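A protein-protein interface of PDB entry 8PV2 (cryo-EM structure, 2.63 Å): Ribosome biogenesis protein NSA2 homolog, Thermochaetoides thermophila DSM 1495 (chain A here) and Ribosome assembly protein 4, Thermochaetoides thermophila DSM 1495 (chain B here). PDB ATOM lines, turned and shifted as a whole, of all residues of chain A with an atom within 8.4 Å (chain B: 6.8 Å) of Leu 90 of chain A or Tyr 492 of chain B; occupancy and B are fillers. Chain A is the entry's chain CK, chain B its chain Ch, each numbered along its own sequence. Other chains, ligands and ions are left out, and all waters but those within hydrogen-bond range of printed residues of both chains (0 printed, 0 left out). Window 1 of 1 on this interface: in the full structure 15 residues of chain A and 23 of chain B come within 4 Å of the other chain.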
ATOM      1  N   PRO A  82      -9.410 -36.221  -1.559  1.00  0.00           N
ATOM      2  CA  PRO A  82      -8.018 -36.631  -1.343  1.00  0.00           C
ATOM      3  C   PRO A  82      -7.427 -36.029  -0.074  1.00  0.00           C
ATOM      4  O   PRO A  82      -8.112 -35.285   0.624  1.00  0.00           O
ATOM      5  CB  PRO A  82      -7.301 -36.107  -2.588  1.00  0.00           C
ATOM      6  CG  PRO A  82      -8.131 -34.967  -3.044  1.00  0.00           C
ATOM      7  CD  PRO A  82      -9.547 -35.326  -2.720  1.00  0.00           C
ATOM      8  N   ASP A  84      -3.621 -34.882   0.337  1.00  0.00           N
ATOM      9  CA  ASP A  84      -2.699 -33.794   0.045  1.00  0.00           C
ATOM     10  C   ASP A  84      -3.355 -32.794  -0.904  1.00  0.00           C
ATOM     11  O   ASP A  84      -4.030 -33.200  -1.853  1.00  0.00           O
ATOM     12  CB  ASP A  84      -1.412 -34.331  -0.576  1.00  0.00           C
ATOM     13  CG  ASP A  84      -0.338 -33.268  -0.712  1.00  0.00           C
ATOM     14  OD1 ASP A  84       0.021 -32.652   0.313  1.00  0.00           O
ATOM     15  OD2 ASP A  84       0.146 -33.043  -1.841  1.00  0.00           O
ATOM     16  N   PRO A  85      -3.193 -31.495  -0.660  1.00  0.00           N
ATOM     17  CA  PRO A  85      -3.737 -30.491  -1.585  1.00  0.00           C
ATOM     18  C   PRO A  85      -3.091 -30.571  -2.961  1.00  0.00           C
ATOM     19  O   PRO A  85      -1.869 -30.510  -3.101  1.00  0.00           O
ATOM     20  CB  PRO A  85      -3.424 -29.166  -0.884  1.00  0.00           C
ATOM     21  CG  PRO A  85      -3.340 -29.521   0.550  1.00  0.00           C
ATOM     22  CD  PRO A  85      -2.739 -30.886   0.601  1.00  0.00           C
ATOM     23  N   ILE A  86      -3.934 -30.711  -3.980  1.00  0.00           N
ATOM     24  CA  ILE A  86      -3.505 -30.814  -5.373  1.00  0.00           C
ATOM     25  C   ILE A  86      -4.334 -29.833  -6.191  1.00  0.00           C
ATOM     26  O   ILE A  86      -5.433 -29.437  -5.775  1.00  0.00           O
ATOM     27  CB  ILE A  86      -3.662 -32.254  -5.915  1.00  0.00           C
ATOM     28  CG1 ILE A  86      -5.073 -32.773  -5.644  1.00  0.00           C
ATOM     29  CG2 ILE A  86      -2.609 -33.163  -5.329  1.00  0.00           C
ATOM     30  CD1 ILE A  86      -5.350 -34.122  -6.227  1.00  0.00           C
ATOM     31  N   PRO A  87      -3.835 -29.410  -7.350  1.00  0.00           N
ATOM     32  CA  PRO A  87      -4.630 -28.524  -8.204  1.00  0.00           C
ATOM     33  C   PRO A  87      -5.784 -29.239  -8.893  1.00  0.00           C
ATOM     34  O   PRO A  87      -5.969 -30.458  -8.801  1.00  0.00           O
ATOM     35  CB  PRO A  87      -3.617 -28.009  -9.231  1.00  0.00           C
ATOM     36  CG  PRO A  87      -2.308 -28.291  -8.669  1.00  0.00           C
ATOM     37  CD  PRO A  87      -2.438 -29.477  -7.799  1.00  0.00           C
ATOM     38  N   SER A  88      -6.569 -28.429  -9.608  1.00  0.00           N
ATOM     39  CA  SER A  88      -7.757 -28.929 -10.286  1.00  0.00           C
ATOM     40  C   SER A  88      -7.411 -29.911 -11.392  1.00  0.00           C
ATOM     41  O   SER A  88      -8.134 -30.890 -11.594  1.00  0.00           O
ATOM     42  CB  SER A  88      -8.559 -27.765 -10.857  1.00  0.00           C
ATOM     43  OG  SER A  88      -9.071 -26.949  -9.825  1.00  0.00           O
ATOM     44  N   TYR A  89      -6.321 -29.672 -12.122  1.00  0.00           N
ATOM     45  CA  TYR A  89      -5.951 -30.593 -13.186  1.00  0.00           C
ATOM     46  C   TYR A  89      -5.400 -31.907 -12.654  1.00  0.00           C
ATOM     47  O   TYR A  89      -5.350 -32.885 -13.406  1.00  0.00           O
ATOM     48  CB  TYR A  89      -4.949 -29.935 -14.139  1.00  0.00           C
ATOM     49  CG  TYR A  89      -3.711 -29.349 -13.501  1.00  0.00           C
ATOM     50  CD1 TYR A  89      -2.598 -30.136 -13.236  1.00  0.00           C
ATOM     51  CD2 TYR A  89      -3.644 -28.001 -13.194  1.00  0.00           C
ATOM     52  CE1 TYR A  89      -1.470 -29.600 -12.666  1.00  0.00           C
ATOM     53  CE2 TYR A  89      -2.517 -27.459 -12.627  1.00  0.00           C
ATOM     54  CZ  TYR A  89      -1.434 -28.263 -12.365  1.00  0.00           C
ATOM     55  OH  TYR A  89      -0.307 -27.723 -11.797  1.00  0.00           O
ATOM     56  N   LEU A  90      -4.995 -31.960 -11.390  1.00  0.00           N
ATOM     57  CA  LEU A  90      -4.598 -33.204 -10.754  1.00  0.00           C
ATOM     58  C   LEU A  90      -5.732 -33.859  -9.984  1.00  0.00           C
ATOM     59  O   LEU A  90      -5.586 -35.008  -9.563  1.00  0.00           O
ATOM     60  CB  LEU A  90      -3.414 -32.969  -9.816  1.00  0.00           C
ATOM     61  CG  LEU A  90      -2.081 -32.641 -10.478  1.00  0.00           C
ATOM     62  CD1 LEU A  90      -0.994 -32.566  -9.434  1.00  0.00           C
ATOM     63  CD2 LEU A  90      -1.745 -33.669 -11.532  1.00  0.00           C
ATOM     64  N   LEU A  91      -6.845 -33.157  -9.782  1.00  0.00           N
ATOM     65  CA  LEU A  91      -8.002 -33.770  -9.144  1.00  0.00           C
ATOM     66  C   LEU A  91      -8.564 -34.907  -9.993  1.00  0.00           C
ATOM     67  O   LEU A  91      -8.460 -34.906 -11.222  1.00  0.00           O
ATOM     68  CB  LEU A  91      -9.094 -32.734  -8.893  1.00  0.00           C
ATOM     69  CG  LEU A  91      -8.884 -31.771  -7.728  1.00  0.00           C
ATOM     70  CD1 LEU A  91      -9.989 -30.748  -7.694  1.00  0.00           C
ATOM     71  CD2 LEU A  91      -8.822 -32.521  -6.421  1.00  0.00           C
ATOM     72  N   ASP A  92      -9.140 -35.897  -9.307  1.00  0.00           N
ATOM     73  CA  ASP A  92      -9.762 -37.115  -9.826  1.00  0.00           C
ATOM     74  C   ASP A  92      -8.787 -38.047 -10.532  1.00  0.00           C
ATOM     75  O   ASP A  92      -9.232 -38.961 -11.232  1.00  0.00           O
ATOM     76  CB  ASP A  92     -10.936 -36.832 -10.776  1.00  0.00           C
ATOM     77  CG  ASP A  92     -12.097 -36.161 -10.082  1.00  0.00           C
ATOM     78  OD1 ASP A  92     -12.618 -35.167 -10.626  1.00  0.00           O
ATOM     79  OD2 ASP A  92     -12.487 -36.624  -8.992  1.00  0.00           O
ATOM     80  N   ARG A  93      -7.485 -37.862 -10.371  1.00  0.00           N
ATOM     81  CA  ARG A  93      -6.495 -38.759 -10.942  1.00  0.00           C
ATOM     82  C   ARG A  93      -5.976 -39.714  -9.877  1.00  0.00           C
ATOM     83  O   ARG A  93      -6.197 -39.527  -8.679  1.00  0.00           O
ATOM     84  CB  ARG A  93      -5.335 -37.974 -11.549  1.00  0.00           C
ATOM     85  CG  ARG A  93      -5.769 -36.966 -12.576  1.00  0.00           C
ATOM     86  CD  ARG A  93      -4.589 -36.346 -13.277  1.00  0.00           C
ATOM     87  NE  ARG A  93      -5.016 -35.534 -14.407  1.00  0.00           N
ATOM     88  CZ  ARG A  93      -5.301 -36.014 -15.607  1.00  0.00           C
ATOM     89  NH1 ARG A  93      -5.199 -37.303 -15.876  1.00  0.00           N
ATOM     90  NH2 ARG A  93      -5.699 -35.180 -16.561  1.00  0.00           N
ATOM     91  N   ALA A  94      -5.286 -40.754 -10.330  1.00  0.00           N
ATOM     92  CA  ALA A  94      -4.683 -41.717  -9.415  1.00  0.00           C
ATOM     93  C   ALA A  94      -3.338 -41.185  -8.940  1.00  0.00           C
ATOM     94  O   ALA A  94      -2.313 -41.389  -9.599  1.00  0.00           O
ATOM     95  CB  ALA A  94      -4.527 -43.070 -10.099  1.00  0.00           C
ATOM     96  N   ASN A  95      -3.335 -40.511  -7.795  1.00  0.00           N
ATOM     97  CA  ASN A  95      -2.126 -39.964  -7.211  1.00  0.00           C
ATOM     98  C   ASN A  95      -1.594 -40.925  -6.158  1.00  0.00           C
ATOM     99  O   ASN A  95      -2.386 -41.636  -5.522  1.00  0.00           O
ATOM    100  CB  ASN A  95      -2.395 -38.588  -6.577  1.00  0.00           C
ATOM    101  CG  ASN A  95      -2.939 -37.579  -7.572  1.00  0.00           C
ATOM    102  OD1 ASN A  95      -3.932 -36.905  -7.309  1.00  0.00           O
ATOM    103  ND2 ASN A  95      -2.277 -37.457  -8.715  1.00  0.00           N
ATOM    104  N   PRO B 148       0.279 -26.538   0.179  1.00  0.00           N
ATOM    105  CA  PRO B 148       0.750 -26.211  -1.175  1.00  0.00           C
ATOM    106  C   PRO B 148      -0.062 -25.125  -1.871  1.00  0.00           C
ATOM    107  O   PRO B 148      -1.274 -25.014  -1.693  1.00  0.00           O
ATOM    108  CB  PRO B 148       0.624 -27.543  -1.914  1.00  0.00           C
ATOM    109  CG  PRO B 148       0.842 -28.540  -0.883  1.00  0.00           C
ATOM    110  CD  PRO B 148       0.225 -28.003   0.362  1.00  0.00           C
ATOM    111  N   ILE B 149       0.640 -24.312  -2.662  1.00  0.00           N
ATOM    112  CA  ILE B 149       0.002 -23.277  -3.464  1.00  0.00           C
ATOM    113  C   ILE B 149      -0.603 -23.906  -4.707  1.00  0.00           C
ATOM    114  O   ILE B 149       0.092 -24.561  -5.493  1.00  0.00           O
ATOM    115  CB  ILE B 149       1.014 -22.189  -3.843  1.00  0.00           C
ATOM    116  CG1 ILE B 149       1.606 -21.557  -2.593  1.00  0.00           C
ATOM    117  CG2 ILE B 149       0.371 -21.139  -4.727  1.00  0.00           C
ATOM    118  CD1 ILE B 149       2.750 -20.674  -2.898  1.00  0.00           C
ATOM    119  N   LEU B 150      -1.902 -23.697  -4.899  1.00  0.00           N
ATOM    120  CA  LEU B 150      -2.628 -24.348  -5.974  1.00  0.00           C
ATOM    121  C   LEU B 150      -2.949 -23.422  -7.134  1.00  0.00           C
ATOM    122  O   LEU B 150      -3.187 -23.910  -8.241  1.00  0.00           O
ATOM    123  CB  LEU B 150      -3.926 -24.964  -5.434  1.00  0.00           C
ATOM    124  CG  LEU B 150      -3.743 -25.771  -4.151  1.00  0.00           C
ATOM    125  CD1 LEU B 150      -5.073 -26.285  -3.635  1.00  0.00           C
ATOM    126  CD2 LEU B 150      -2.773 -26.908  -4.367  1.00  0.00           C
ATOM    127  N   SER B 151      -2.956 -22.110  -6.919  1.00  0.00           N
ATOM    128  CA  SER B 151      -3.205 -21.193  -8.022  1.00  0.00           C
ATOM    129  C   SER B 151      -2.471 -19.889  -7.757  1.00  0.00           C
ATOM    130  O   SER B 151      -2.270 -19.509  -6.606  1.00  0.00           O
ATOM    131  CB  SER B 151      -4.707 -20.947  -8.200  1.00  0.00           C
ATOM    132  OG  SER B 151      -4.978 -20.180  -9.357  1.00  0.00           O
ATOM    133  N   CYS B 152      -2.071 -19.209  -8.832  1.00  0.00           N
ATOM    134  CA  CYS B 152      -1.472 -17.886  -8.713  1.00  0.00           C
ATOM    135  C   CYS B 152      -1.829 -17.069  -9.944  1.00  0.00           C
ATOM    136  O   CYS B 152      -2.049 -17.628 -11.020  1.00  0.00           O
ATOM    137  CB  CYS B 152       0.052 -17.947  -8.560  1.00  0.00           C
ATOM    138  SG  CYS B 152       0.963 -18.378 -10.051  1.00  0.00           S
ATOM    139  N   ASN B 408      -1.416 -31.365 -20.586  1.00  0.00           N
ATOM    140  CA  ASN B 408      -1.965 -30.733 -19.398  1.00  0.00           C
ATOM    141  C   ASN B 408      -2.429 -29.303 -19.642  1.00  0.00           C
ATOM    142  O   ASN B 408      -3.536 -28.938 -19.241  1.00  0.00           O
ATOM    143  CB  ASN B 408      -0.924 -30.766 -18.279  1.00  0.00           C
ATOM    144  CG  ASN B 408      -1.532 -30.557 -16.923  1.00  0.00           C
ATOM    145  OD1 ASN B 408      -2.311 -31.378 -16.449  1.00  0.00           O
ATOM    146  ND2 ASN B 408      -1.178 -29.456 -16.282  1.00  0.00           N
ATOM    147  N   TRP B 424       2.666 -34.381 -20.404  1.00  0.00           N
ATOM    148  CA  TRP B 424       3.169 -35.306 -19.402  1.00  0.00           C
ATOM    149  C   TRP B 424       4.310 -36.159 -19.922  1.00  0.00           C
ATOM    150  O   TRP B 424       4.835 -36.993 -19.181  1.00  0.00           O
ATOM    151  CB  TRP B 424       2.042 -36.206 -18.895  1.00  0.00           C
ATOM    152  CG  TRP B 424       1.054 -35.526 -18.011  1.00  0.00           C
ATOM    153  CD1 TRP B 424       0.357 -34.387 -18.278  1.00  0.00           C
ATOM    154  CD2 TRP B 424       0.626 -35.962 -16.719  1.00  0.00           C
ATOM    155  NE1 TRP B 424      -0.468 -34.078 -17.229  1.00  0.00           N
ATOM    156  CE2 TRP B 424      -0.320 -35.031 -16.258  1.00  0.00           C
ATOM    157  CE3 TRP B 424       0.959 -37.043 -15.904  1.00  0.00           C
ATOM    158  CZ2 TRP B 424      -0.938 -35.152 -15.022  1.00  0.00           C
ATOM    159  CZ3 TRP B 424       0.347 -37.159 -14.680  1.00  0.00           C
ATOM    160  CH2 TRP B 424      -0.591 -36.221 -14.251  1.00  0.00           C
ATOM    161  N   TYR B 450       3.614 -29.124 -15.985  1.00  0.00           N
ATOM    162  CA  TYR B 450       2.244 -28.831 -15.599  1.00  0.00           C
ATOM    163  C   TYR B 450       1.723 -27.533 -16.185  1.00  0.00           C
ATOM    164  O   TYR B 450       0.581 -27.507 -16.654  1.00  0.00           O
ATOM    165  CB  TYR B 450       2.096 -28.801 -14.077  1.00  0.00           C
ATOM    166  CG  TYR B 450       2.201 -30.162 -13.441  1.00  0.00           C
ATOM    167  CD1 TYR B 450       1.820 -31.299 -14.133  1.00  0.00           C
ATOM    168  CD2 TYR B 450       2.650 -30.307 -12.142  1.00  0.00           C
ATOM    169  CE1 TYR B 450       1.912 -32.541 -13.560  1.00  0.00           C
ATOM    170  CE2 TYR B 450       2.736 -31.546 -11.557  1.00  0.00           C
ATOM    171  CZ  TYR B 450       2.369 -32.660 -12.272  1.00  0.00           C
ATOM    172  OH  TYR B 450       2.456 -33.898 -11.689  1.00  0.00           O
ATOM    173  N   GLN B 451       2.500 -26.449 -16.182  1.00  0.00           N
ATOM    174  CA  GLN B 451       1.961 -25.247 -16.810  1.00  0.00           C
ATOM    175  C   GLN B 451       2.985 -24.566 -17.697  1.00  0.00           C
ATOM    176  O   GLN B 451       4.191 -24.774 -17.574  1.00  0.00           O
ATOM    177  CB  GLN B 451       1.420 -24.221 -15.807  1.00  0.00           C
ATOM    178  CG  GLN B 451       0.168 -24.644 -15.078  1.00  0.00           C
ATOM    179  CD  GLN B 451      -0.339 -23.574 -14.153  1.00  0.00           C
ATOM    180  OE1 GLN B 451       0.274 -22.519 -14.014  1.00  0.00           O
ATOM    181  NE2 GLN B 451      -1.471 -23.833 -13.514  1.00  0.00           N
ATOM    182  N   GLY B 464       6.590 -24.510 -16.008  1.00  0.00           N
ATOM    183  CA  GLY B 464       6.809 -25.039 -14.683  1.00  0.00           C
ATOM    184  C   GLY B 464       6.431 -26.495 -14.607  1.00  0.00           C
ATOM    185  O   GLY B 464       5.322 -26.877 -15.021  1.00  0.00           O
ATOM    186  N   SER B 465       7.341 -27.315 -14.084  1.00  0.00           N
ATOM    187  CA  SER B 465       7.159 -28.755 -14.160  1.00  0.00           C
ATOM    188  C   SER B 465       7.180 -29.413 -12.788  1.00  0.00           C
ATOM    189  O   SER B 465       7.328 -28.768 -11.749  1.00  0.00           O
ATOM    190  CB  SER B 465       8.227 -29.395 -15.045  1.00  0.00           C
ATOM    191  OG  SER B 465       8.169 -30.804 -14.959  1.00  0.00           O
ATOM    192  N   HIS B 487      12.777 -24.331  -6.272  1.00  0.00           N
ATOM    193  CA  HIS B 487      11.674 -24.981  -5.581  1.00  0.00           C
ATOM    194  C   HIS B 487      12.126 -26.319  -5.013  1.00  0.00           C
ATOM    195  O   HIS B 487      12.791 -27.103  -5.691  1.00  0.00           O
ATOM    196  CB  HIS B 487      10.490 -25.186  -6.528  1.00  0.00           C
ATOM    197  CG  HIS B 487       9.620 -23.978  -6.686  1.00  0.00           C
ATOM    198  ND1 HIS B 487       8.612 -23.667  -5.801  1.00  0.00           N
ATOM    199  CD2 HIS B 487       9.609 -23.004  -7.624  1.00  0.00           C
ATOM    200  CE1 HIS B 487       8.015 -22.556  -6.189  1.00  0.00           C
ATOM    201  NE2 HIS B 487       8.602 -22.133  -7.292  1.00  0.00           N
ATOM    202  N   ASP B 489      10.033 -28.651  -4.141  1.00  0.00           N
ATOM    203  CA  ASP B 489       9.048 -29.656  -4.505  1.00  0.00           C
ATOM    204  C   ASP B 489       8.365 -29.204  -5.791  1.00  0.00           C
ATOM    205  O   ASP B 489       8.818 -28.267  -6.453  1.00  0.00           O
ATOM    206  CB  ASP B 489       8.078 -29.895  -3.345  1.00  0.00           C
ATOM    207  CG  ASP B 489       7.715 -31.354  -3.189  1.00  0.00           C
ATOM    208  OD1 ASP B 489       7.909 -32.118  -4.157  1.00  0.00           O
ATOM    209  OD2 ASP B 489       7.253 -31.742  -2.096  1.00  0.00           O
ATOM    210  N   GLU B 490       7.274 -29.882  -6.148  1.00  0.00           N
ATOM    211  CA  GLU B 490       6.651 -29.700  -7.455  1.00  0.00           C
ATOM    212  C   GLU B 490       6.062 -28.307  -7.607  1.00  0.00           C
ATOM    213  O   GLU B 490       5.572 -27.712  -6.646  1.00  0.00           O
ATOM    214  CB  GLU B 490       5.558 -30.743  -7.667  1.00  0.00           C
ATOM    215  CG  GLU B 490       6.013 -32.163  -7.442  1.00  0.00           C
ATOM    216  CD  GLU B 490       4.905 -33.170  -7.652  1.00  0.00           C
ATOM    217  OE1 GLU B 490       3.875 -32.807  -8.254  1.00  0.00           O
ATOM    218  OE2 GLU B 490       5.065 -34.328  -7.218  1.00  0.00           O
ATOM    219  N   VAL B 491       6.118 -27.786  -8.826  1.00  0.00           N
ATOM    220  CA  VAL B 491       5.599 -26.461  -9.132  1.00  0.00           C
ATOM    221  C   VAL B 491       4.220 -26.613  -9.753  1.00  0.00           C
ATOM    222  O   VAL B 491       4.078 -27.189 -10.837  1.00  0.00           O
ATOM    223  CB  VAL B 491       6.548 -25.702 -10.072  1.00  0.00           C
ATOM    224  CG1 VAL B 491       5.977 -24.345 -10.402  1.00  0.00           C
ATOM    225  CG2 VAL B 491       7.917 -25.568  -9.446  1.00  0.00           C
ATOM    226  N   TYR B 492       3.205 -26.083  -9.076  1.00  0.00           N
ATOM    227  CA  TYR B 492       1.819 -26.248  -9.488  1.00  0.00           C
ATOM    228  C   TYR B 492       1.275 -25.090 -10.302  1.00  0.00           C
ATOM    229  O   TYR B 492       0.544 -25.323 -11.263  1.00  0.00           O
ATOM    230  CB  TYR B 492       0.918 -26.438  -8.265  1.00  0.00           C
ATOM    231  CG  TYR B 492       1.029 -27.786  -7.608  1.00  0.00           C
ATOM    232  CD1 TYR B 492       1.325 -28.917  -8.350  1.00  0.00           C
ATOM    233  CD2 TYR B 492       0.807 -27.934  -6.249  1.00  0.00           C
ATOM    234  CE1 TYR B 492       1.416 -30.151  -7.755  1.00  0.00           C
ATOM    235  CE2 TYR B 492       0.893 -29.164  -5.647  1.00  0.00           C
ATOM    236  CZ  TYR B 492       1.197 -30.269  -6.405  1.00  0.00           C
ATOM    237  OH  TYR B 492       1.284 -31.501  -5.807  1.00  0.00           O
ATOM    238  N   ALA B 493       1.610 -23.855  -9.947  1.00  0.00           N
ATOM    239  CA  ALA B 493       1.050 -22.673 -10.580  1.00  0.00           C
ATOM    240  C   ALA B 493       2.168 -21.774 -11.080  1.00  0.00           C
ATOM    241  O   ALA B 493       3.126 -21.501 -10.354  1.00  0.00           O
ATOM    242  CB  ALA B 493       0.158 -21.911  -9.606  1.00  0.00           C
ATOM    243  N   VAL B 494       2.051 -21.333 -12.332  1.00  0.00           N
ATOM    244  CA  VAL B 494       3.033 -20.472 -12.984  1.00  0.00           C
ATOM    245  C   VAL B 494       2.290 -19.345 -13.693  1.00  0.00           C
ATOM    246  O   VAL B 494       1.312 -19.591 -14.405  1.00  0.00           O
ATOM    247  CB  VAL B 494       3.905 -21.261 -13.989  1.00  0.00           C
ATOM    248  CG1 VAL B 494       4.830 -20.343 -14.746  1.00  0.00           C
ATOM    249  CG2 VAL B 494       4.709 -22.325 -13.290  1.00  0.00           C
ATOM    250  N   SER B 505       5.750 -18.275  -9.350  1.00  0.00           N
ATOM    251  CA  SER B 505       5.582 -19.713  -9.284  1.00  0.00           C
ATOM    252  C   SER B 505       5.206 -20.107  -7.865  1.00  0.00           C
ATOM    253  O   SER B 505       5.606 -19.466  -6.890  1.00  0.00           O
ATOM    254  CB  SER B 505       6.847 -20.448  -9.719  1.00  0.00           C
ATOM    255  OG  SER B 505       7.985 -19.945  -9.052  1.00  0.00           O
ATOM    256  N   GLY B 506       4.408 -21.154  -7.768  1.00  0.00           N
ATOM    257  CA  GLY B 506       4.020 -21.696  -6.479  1.00  0.00           C
ATOM    258  C   GLY B 506       3.744 -23.170  -6.614  1.00  0.00           C
ATOM    259  O   GLY B 506       3.426 -23.662  -7.698  1.00  0.00           O
ATOM    260  N   GLY B 507       3.865 -23.884  -5.505  1.00  0.00           N
ATOM    261  CA  GLY B 507       3.641 -25.310  -5.560  1.00  0.00           C
ATOM    262  C   GLY B 507       3.649 -26.010  -4.223  1.00  0.00           C
ATOM    263  O   GLY B 507       3.202 -25.462  -3.215  1.00  0.00           O
ATOM    264  N   LYS B 508       4.179 -27.229  -4.215  1.00  0.00           N
ATOM    265  CA  LYS B 508       4.117 -28.106  -3.055  1.00  0.00           C
ATOM    266  C   LYS B 508       5.012 -27.657  -1.905  1.00  0.00           C
ATOM    267  O   LYS B 508       4.833 -28.138  -0.783  1.00  0.00           O
ATOM    268  CB  LYS B 508       4.488 -29.520  -3.490  1.00  0.00           C
ATOM    269  CG  LYS B 508       3.834 -30.634  -2.728  1.00  0.00           C
ATOM    270  CD  LYS B 508       4.169 -31.954  -3.390  1.00  0.00           C
ATOM    271  CE  LYS B 508       3.756 -33.129  -2.539  1.00  0.00           C
ATOM    272  NZ  LYS B 508       4.228 -34.404  -3.136  1.00  0.00           N
ATOM    273  N   ASP B 509       5.960 -26.750  -2.145  1.00  0.00           N
ATOM    274  CA  ASP B 509       6.864 -26.326  -1.080  1.00  0.00           C
ATOM    275  C   ASP B 509       6.346 -25.130  -0.291  1.00  0.00           C
ATOM    276  O   ASP B 509       7.102 -24.574   0.511  1.00  0.00           O
ATOM    277  CB  ASP B 509       8.247 -26.008  -1.645  1.00  0.00           C
ATOM    278  CG  ASP B 509       8.201 -25.037  -2.798  1.00  0.00           C
ATOM    279  OD1 ASP B 509       7.092 -24.678  -3.244  1.00  0.00           O
ATOM    280  OD2 ASP B 509       9.283 -24.615  -3.250  1.00  0.00           O
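CE of Lys 508 of chain B touches OD2 of Asp 84 of chain A, at 3.7 Å.
Pro 148 of chain B touches Pro 85 of chain A.
Leu 150 of chain B touches Pro 85 of chain A (CD2 to O, 3.9 Å).
C of Ile 86 of chain A touches CD2 of Leu 150 of chain B (3.8 Å).
Pro 87 of chain A touches Tyr 492 of chain B (CG to CG, 3.5 Å).
CD1 of Tyr 89 of chain A touches ND2 of Asn 408 of chain B, at 3.4 Å.
Tyr 450 of chain B touches Tyr 89 of chain A (CB to OH, 3.5 Å).
Tyr 89 of chain A touches Gln 451 of chain B (CE2 to NE2, 3.9 Å).
CD2 of Leu 90 of chain A touches CZ2 of Trp 424 of chain B, 3.9 Å away.
Leu 90 of chain A touches Tyr 492 of chain B (CD1 to CE1, 3.8 Å).
Of the 13 printed residues of chain A, 6 touch a printed residue of chain B.
Of the 23 printed residues of chain B, 8 touch a printed residue of chain A.
Hydrophobic or aromatic side chains of chain B within 4 Å of the printed part of chain A: Pro 148, Leu 150, Trp 424, Tyr 450 and Tyr 492.
Among the printed residues, no Asp or Glu carboxylate lies within 4 Å of a Lys or Arg side-chain nitrogen of the other chain.
The backbone NH (N) of Lys 508 of chain B sits at hydrogen-bond distance from the backbone carbonyl oxygen (O) of Glu 490 of chain B, 2.8 Å away.
O of Tyr 492 of chain B lies within hydrogen-bond range of NE2 of Gln 451 of chain B, at 3.4 Å.
The side-chain amide nitrogen (ND2) of Asn 408 of chain B is in hydrogen-bond range of the backbone carbonyl oxygen (O) of Tyr 450 of chain B (2.7 Å).
The backbone carbonyl oxygen of Gln 451 of chain B is in hydrogen-bond range of the backbone NH of Gly 464 of chain B, 2.9 Å away.
O of Tyr 89 of chain A lies within hydrogen-bond range of NE of Arg 93 of chain A, 2.9 Å away.
The side-chain amide oxygen (OD1) of Asn 408 of chain B is in hydrogen-bond range of the indole nitrogen (NE1) of Trp 424 of chain B, 3.4 Å away.
Of chain B, only Trp 424 and Tyr 492 come within 4 Å of Leu 90 of chain A.
Of the printed residues of chain A, Tyr 492 of chain B touches Pro 85, Pro 87, Tyr 89 and Leu 90.
Printed residues of chain A within 4 Å of Gln 451 of chain B: Tyr 89 (3.9 Å).
Printed residues of chain B within 4 Å of Ile 86 of chain A: Leu 150.
Printed residues of chain A within 4 Å of Tyr 450 of chain B: Tyr 89.
Gly 506 of chain B touches none of the printed residues of chain A.
The nearest residue of chain B that does not touch Leu 90 of chain A is Tyr 450 of chain B (4.2 Å).
The nearest printed residue of chain A that does not touch Tyr 492 of chain B is Ile 86 of chain A (4.3 Å).
The backbone carbonyl oxygen of Tyr 492 of chain B lies within hydrogen-bond range of the side-chain hydroxyl of Tyr 89 of chain A (2.6 Å).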
